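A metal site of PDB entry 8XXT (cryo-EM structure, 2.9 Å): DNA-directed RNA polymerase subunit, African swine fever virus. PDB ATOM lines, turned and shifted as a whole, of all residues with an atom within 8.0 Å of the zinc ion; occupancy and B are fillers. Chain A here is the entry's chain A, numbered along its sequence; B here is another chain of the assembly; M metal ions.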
ATOM      1  N   ILE A  98     -17.439 -13.010 -16.057  1.00  0.00           N
ATOM      2  CA  ILE A  98     -16.064 -13.123 -15.575  1.00  0.00           C
ATOM      3  C   ILE A  98     -15.817 -14.544 -15.072  1.00  0.00           C
ATOM      4  O   ILE A  98     -16.743 -15.259 -14.673  1.00  0.00           O
ATOM      5  CB  ILE A  98     -15.754 -12.098 -14.471  1.00  0.00           C
ATOM      6  CG1 ILE A  98     -16.630 -12.385 -13.247  1.00  0.00           C
ATOM      7  CG2 ILE A  98     -15.973 -10.695 -14.988  1.00  0.00           C
ATOM      8  CD1 ILE A  98     -16.733 -11.243 -12.284  1.00  0.00           C
ATOM      9  N   CYS A  99     -14.551 -14.936 -15.101  1.00  0.00           N
ATOM     10  CA  CYS A  99     -14.156 -16.243 -14.581  1.00  0.00           C
ATOM     11  C   CYS A  99     -14.127 -16.179 -13.060  1.00  0.00           C
ATOM     12  O   CYS A  99     -13.452 -15.337 -12.479  1.00  0.00           O
ATOM     13  CB  CYS A  99     -12.788 -16.635 -15.132  1.00  0.00           C
ATOM     14  SG  CYS A  99     -12.172 -18.226 -14.553  1.00  0.00           S
ATOM     15  N   LEU A 100     -14.865 -17.091 -12.425  1.00  0.00           N
ATOM     16  CA  LEU A 100     -14.979 -17.073 -10.970  1.00  0.00           C
ATOM     17  C   LEU A 100     -13.690 -17.458 -10.277  1.00  0.00           C
ATOM     18  O   LEU A 100     -13.574 -17.302  -9.054  1.00  0.00           O
ATOM     19  CB  LEU A 100     -16.106 -17.992 -10.522  1.00  0.00           C
ATOM     20  CG  LEU A 100     -17.517 -17.406 -10.464  1.00  0.00           C
ATOM     21  CD1 LEU A 100     -18.099 -17.221 -11.856  1.00  0.00           C
ATOM     22  CD2 LEU A 100     -18.423 -18.280  -9.623  1.00  0.00           C
ATOM     23  N   ASN A 101     -12.692 -17.967 -11.014  1.00  0.00           N
ATOM     24  CA  ASN A 101     -11.446 -18.403 -10.408  1.00  0.00           C
ATOM     25  C   ASN A 101     -10.267 -17.492 -10.704  1.00  0.00           C
ATOM     26  O   ASN A 101      -9.362 -17.392  -9.871  1.00  0.00           O
ATOM     27  CB  ASN A 101     -11.108 -19.824 -10.880  1.00  0.00           C
ATOM     28  CG  ASN A 101     -11.979 -20.874 -10.228  1.00  0.00           C
ATOM     29  OD1 ASN A 101     -11.894 -21.099  -9.026  1.00  0.00           O
ATOM     30  ND2 ASN A 101     -12.822 -21.522 -11.021  1.00  0.00           N
ATOM     31  N   CYS A 102     -10.248 -16.826 -11.854  1.00  0.00           N
ATOM     32  CA  CYS A 102      -9.121 -15.979 -12.212  1.00  0.00           C
ATOM     33  C   CYS A 102      -9.490 -14.546 -12.532  1.00  0.00           C
ATOM     34  O   CYS A 102      -8.593 -13.737 -12.799  1.00  0.00           O
ATOM     35  CB  CYS A 102      -8.366 -16.577 -13.404  1.00  0.00           C
ATOM     36  SG  CYS A 102      -9.015 -16.065 -15.002  1.00  0.00           S
ATOM     37  N   GLY A 103     -10.784 -14.191 -12.528  1.00  0.00           N
ATOM     38  CA  GLY A 103     -11.207 -12.832 -12.758  1.00  0.00           C
ATOM     39  C   GLY A 103     -11.212 -12.382 -14.196  1.00  0.00           C
ATOM     40  O   GLY A 103     -11.912 -11.412 -14.520  1.00  0.00           O
ATOM     41  N   ALA A 104     -10.456 -13.031 -15.078  1.00  0.00           N
ATOM     42  CA  ALA A 104     -10.449 -12.646 -16.474  1.00  0.00           C
ATOM     43  C   ALA A 104     -11.809 -12.947 -17.109  1.00  0.00           C
ATOM     44  O   ALA A 104     -12.472 -13.914 -16.729  1.00  0.00           O
ATOM     45  CB  ALA A 104      -9.346 -13.371 -17.237  1.00  0.00           C
ATOM     46  N   PRO A 105     -12.243 -12.129 -18.063  1.00  0.00           N
ATOM     47  CA  PRO A 105     -13.556 -12.360 -18.676  1.00  0.00           C
ATOM     48  C   PRO A 105     -13.573 -13.637 -19.485  1.00  0.00           C
ATOM     49  O   PRO A 105     -12.629 -13.948 -20.209  1.00  0.00           O
ATOM     50  CB  PRO A 105     -13.748 -11.120 -19.561  1.00  0.00           C
ATOM     51  CG  PRO A 105     -12.359 -10.702 -19.894  1.00  0.00           C
ATOM     52  CD  PRO A 105     -11.538 -10.988 -18.679  1.00  0.00           C
ATOM     53  N   ILE A 106     -14.675 -14.382 -19.365  1.00  0.00           N
ATOM     54  CA  ILE A 106     -14.843 -15.595 -20.158  1.00  0.00           C
ATOM     55  C   ILE A 106     -15.341 -15.276 -21.558  1.00  0.00           C
ATOM     56  O   ILE A 106     -15.167 -16.100 -22.469  1.00  0.00           O
ATOM     57  CB  ILE A 106     -15.808 -16.573 -19.457  1.00  0.00           C
ATOM     58  CG1 ILE A 106     -17.246 -16.078 -19.563  1.00  0.00           C
ATOM     59  CG2 ILE A 106     -15.401 -16.770 -18.016  1.00  0.00           C
ATOM     60  CD1 ILE A 106     -18.189 -16.738 -18.583  1.00  0.00           C
ATOM     61  N   LYS A 132     -18.192 -22.741 -20.055  1.00  0.00           N
ATOM     62  CA  LYS A 132     -17.085 -22.286 -20.887  1.00  0.00           C
ATOM     63  C   LYS A 132     -15.760 -22.521 -20.181  1.00  0.00           C
ATOM     64  O   LYS A 132     -15.656 -22.456 -18.952  1.00  0.00           O
ATOM     65  CB  LYS A 132     -17.250 -20.803 -21.231  1.00  0.00           C
ATOM     66  CG  LYS A 132     -16.578 -20.401 -22.532  1.00  0.00           C
ATOM     67  CD  LYS A 132     -17.029 -19.024 -22.987  1.00  0.00           C
ATOM     68  CE  LYS A 132     -16.438 -18.668 -24.335  1.00  0.00           C
ATOM     69  NZ  LYS A 132     -16.659 -17.245 -24.696  1.00  0.00           N
ATOM     70  N   GLN A 133     -14.727 -22.800 -20.971  1.00  0.00           N
ATOM     71  CA  GLN A 133     -13.401 -23.070 -20.455  1.00  0.00           C
ATOM     72  C   GLN A 133     -12.556 -21.806 -20.515  1.00  0.00           C
ATOM     73  O   GLN A 133     -12.371 -21.216 -21.591  1.00  0.00           O
ATOM     74  CB  GLN A 133     -12.732 -24.188 -21.247  1.00  0.00           C
ATOM     75  CG  GLN A 133     -11.656 -24.951 -20.489  1.00  0.00           C
ATOM     76  CD  GLN A 133     -11.953 -25.053 -19.004  1.00  0.00           C
ATOM     77  OE1 GLN A 133     -11.418 -24.305 -18.201  1.00  0.00           O
ATOM     78  NE2 GLN A 133     -12.823 -25.984 -18.643  1.00  0.00           N
ATOM     79  N   CYS A 134     -12.036 -21.386 -19.364  1.00  0.00           N
ATOM     80  CA  CYS A 134     -11.248 -20.160 -19.307  1.00  0.00           C
ATOM     81  C   CYS A 134      -9.893 -20.374 -19.984  1.00  0.00           C
ATOM     82  O   CYS A 134      -9.248 -21.407 -19.808  1.00  0.00           O
ATOM     83  CB  CYS A 134     -11.042 -19.727 -17.860  1.00  0.00           C
ATOM     84  SG  CYS A 134      -9.921 -18.333 -17.693  1.00  0.00           S
ATOM     85  N   TYR A 135      -9.462 -19.364 -20.742  1.00  0.00           N
ATOM     86  CA  TYR A 135      -8.247 -19.486 -21.534  1.00  0.00           C
ATOM     87  C   TYR A 135      -6.986 -19.337 -20.691  1.00  0.00           C
ATOM     88  O   TYR A 135      -5.979 -19.998 -20.960  1.00  0.00           O
ATOM     89  CB  TYR A 135      -8.238 -18.461 -22.659  1.00  0.00           C
ATOM     90  CG  TYR A 135      -9.622 -18.021 -23.098  1.00  0.00           C
ATOM     91  CD1 TYR A 135     -10.528 -18.925 -23.646  1.00  0.00           C
ATOM     92  CD2 TYR A 135     -10.021 -16.696 -22.983  1.00  0.00           C
ATOM     93  CE1 TYR A 135     -11.784 -18.527 -24.045  1.00  0.00           C
ATOM     94  CE2 TYR A 135     -11.278 -16.288 -23.381  1.00  0.00           C
ATOM     95  CZ  TYR A 135     -12.153 -17.214 -23.911  1.00  0.00           C
ATOM     96  OH  TYR A 135     -13.409 -16.806 -24.309  1.00  0.00           O
ATOM     97  N   VAL A 136      -7.021 -18.482 -19.671  1.00  0.00           N
ATOM     98  CA  VAL A 136      -5.789 -18.124 -18.965  1.00  0.00           C
ATOM     99  C   VAL A 136      -5.553 -18.949 -17.700  1.00  0.00           C
ATOM    100  O   VAL A 136      -4.421 -18.998 -17.218  1.00  0.00           O
ATOM    101  CB  VAL A 136      -5.782 -16.636 -18.617  1.00  0.00           C
ATOM    102  CG1 VAL A 136      -5.319 -15.820 -19.814  1.00  0.00           C
ATOM    103  CG2 VAL A 136      -7.148 -16.182 -18.158  1.00  0.00           C
ATOM    104  N   CYS A 137      -6.595 -19.577 -17.144  1.00  0.00           N
ATOM    105  CA  CYS A 137      -6.422 -20.384 -15.950  1.00  0.00           C
ATOM    106  C   CYS A 137      -7.050 -21.762 -16.047  1.00  0.00           C
ATOM    107  O   CYS A 137      -6.963 -22.531 -15.085  1.00  0.00           O
ATOM    108  CB  CYS A 137      -6.977 -19.653 -14.717  1.00  0.00           C
ATOM    109  SG  CYS A 137      -8.747 -19.852 -14.450  1.00  0.00           S
ATOM    110  N   LYS A 138      -7.677 -22.097 -17.177  1.00  0.00           N
ATOM    111  CA  LYS A 138      -8.172 -23.449 -17.447  1.00  0.00           C
ATOM    112  C   LYS A 138      -9.136 -23.921 -16.371  1.00  0.00           C
ATOM    113  O   LYS A 138      -9.125 -25.083 -15.968  1.00  0.00           O
ATOM    114  CB  LYS A 138      -7.006 -24.433 -17.602  1.00  0.00           C
ATOM    115  CG  LYS A 138      -6.008 -24.069 -18.694  1.00  0.00           C
ATOM    116  CD  LYS A 138      -6.686 -23.474 -19.921  1.00  0.00           C
ATOM    117  CE  LYS A 138      -6.130 -24.077 -21.205  1.00  0.00           C
ATOM    118  NZ  LYS A 138      -6.344 -23.174 -22.371  1.00  0.00           N
ATOM    119  N   ALA A 139      -9.996 -23.019 -15.906  1.00  0.00           N
ATOM    120  CA  ALA A 139     -11.056 -23.346 -14.958  1.00  0.00           C
ATOM    121  C   ALA A 139     -12.405 -23.167 -15.629  1.00  0.00           C
ATOM    122  O   ALA A 139     -12.657 -22.135 -16.251  1.00  0.00           O
ATOM    123  CB  ALA A 139     -10.961 -22.488 -13.698  1.00  0.00           C
ATOM    124  N   VAL A 140     -13.264 -24.168 -15.498  1.00  0.00           N
ATOM    125  CA  VAL A 140     -14.560 -24.158 -16.178  1.00  0.00           C
ATOM    126  C   VAL A 140     -15.475 -23.167 -15.483  1.00  0.00           C
ATOM    127  O   VAL A 140     -15.581 -23.149 -14.249  1.00  0.00           O
ATOM    128  CB  VAL A 140     -15.170 -25.565 -16.210  1.00  0.00           C
ATOM    129  CG1 VAL A 140     -15.149 -26.190 -14.821  1.00  0.00           C
ATOM    130  CG2 VAL A 140     -16.588 -25.525 -16.759  1.00  0.00           C
ATOM    131  N   HIS A 141     -16.124 -22.317 -16.267  1.00  0.00           N
ATOM    132  CA  HIS A 141     -17.047 -21.329 -15.701  1.00  0.00           C
ATOM    133  C   HIS A 141     -18.369 -21.998 -15.360  1.00  0.00           C
ATOM    134  O   HIS A 141     -18.978 -22.640 -16.217  1.00  0.00           O
ATOM    135  CB  HIS A 141     -17.276 -20.180 -16.668  1.00  0.00           C
ATOM    136  CG  HIS A 141     -18.275 -19.174 -16.177  1.00  0.00           C
ATOM    137  ND1 HIS A 141     -19.599 -19.181 -16.585  1.00  0.00           N
ATOM    138  CD2 HIS A 141     -18.155 -18.155 -15.300  1.00  0.00           C
ATOM    139  CE1 HIS A 141     -20.238 -18.198 -15.985  1.00  0.00           C
ATOM    140  NE2 HIS A 141     -19.389 -17.559 -15.205  1.00  0.00           N
ATOM    141  N   ARG A 176     -11.238  -9.769  -7.948  1.00  0.00           N
ATOM    142  CA  ARG A 176     -10.336 -10.349  -8.937  1.00  0.00           C
ATOM    143  C   ARG A 176     -10.424  -9.650 -10.289  1.00  0.00           C
ATOM    144  O   ARG A 176      -9.532  -9.858 -11.121  1.00  0.00           O
ATOM    145  CB  ARG A 176     -10.644 -11.841  -9.094  1.00  0.00           C
ATOM    146  CG  ARG A 176      -9.450 -12.664  -9.547  1.00  0.00           C
ATOM    147  CD  ARG A 176      -9.615 -14.135  -9.216  1.00  0.00           C
ATOM    148  NE  ARG A 176     -10.159 -14.356  -7.883  1.00  0.00           N
ATOM    149  CZ  ARG A 176     -11.250 -15.049  -7.619  1.00  0.00           C
ATOM    150  NH1 ARG A 176     -11.956 -15.609  -8.590  1.00  0.00           N
ATOM    151  NH2 ARG A 176     -11.646 -15.195  -6.360  1.00  0.00           N
ATOM    152  N   HIS B  37      -3.274 -10.959 -17.867  1.00  0.00           N
ATOM    153  CA  HIS B  37      -3.956 -10.479 -16.677  1.00  0.00           C
ATOM    154  C   HIS B  37      -4.774 -11.595 -16.043  1.00  0.00           C
ATOM    155  O   HIS B  37      -5.627 -12.188 -16.717  1.00  0.00           O
ATOM    156  CB  HIS B  37      -4.861  -9.292 -17.009  1.00  0.00           C
ATOM    157  CG  HIS B  37      -4.193  -7.957 -16.879  1.00  0.00           C
ATOM    158  ND1 HIS B  37      -4.632  -6.844 -17.545  1.00  0.00           N
ATOM    159  CD2 HIS B  37      -3.140  -7.560 -16.126  1.00  0.00           C
ATOM    160  CE1 HIS B  37      -3.864  -5.813 -17.231  1.00  0.00           C
ATOM    161  NE2 HIS B  37      -2.961  -6.221 -16.370  1.00  0.00           N
ATOM    162  N   LEU B  38      -4.514 -11.865 -14.766  1.00  0.00           N
ATOM    163  CA  LEU B  38      -5.424 -12.620 -13.910  1.00  0.00           C
ATOM    164  C   LEU B  38      -5.003 -12.361 -12.475  1.00  0.00           C
ATOM    165  O   LEU B  38      -3.855 -12.608 -12.099  1.00  0.00           O
ATOM    166  CB  LEU B  38      -5.420 -14.121 -14.231  1.00  0.00           C
ATOM    167  CG  LEU B  38      -4.148 -14.974 -14.208  1.00  0.00           C
ATOM    168  CD1 LEU B  38      -3.953 -15.660 -12.856  1.00  0.00           C
ATOM    169  CD2 LEU B  38      -4.174 -15.998 -15.332  1.00  0.00           C
HETATM  170 ZN    ZN M   1      -9.994 -18.133 -15.383  1.00  0.00          ZN
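SG of Cys 102 binds the zinc ion. SG of Cys 134 binds the zinc ion (2.3 Å). SG of Cys 137 binds the zinc ion, 2.3 Å away. The zinc ion is bound by SG of Cys 99, 2.3 Å away.
N of Cys 134 sits at hydrogen-bond distance from O of Ala 139 (3.3 Å). The side-chain sulfur of Cys 102 lies close to the backbone NH of Ala 104 (3.4 Å). The backbone NH (N) of Asn 101 sits close to the side-chain sulfur (SG) of Cys 99, at 3.6 Å. The backbone NH (N) of Val 136 lies close to the side-chain sulfur (SG) of Cys 134. The backbone NH (N) of Cys 99 is in hydrogen-bond range of the backbone carbonyl oxygen (O) of Ala 104 (2.8 Å). The side-chain sulfur (SG) of Cys 137 lies close to the backbone NH (N) of Ala 139 (3.7 Å).
Of the 22 residues printed, 4 come within 4 Å of the zinc ion. The nearest printed residue that does not touch the zinc ion is Val 136 (4.4 Å).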
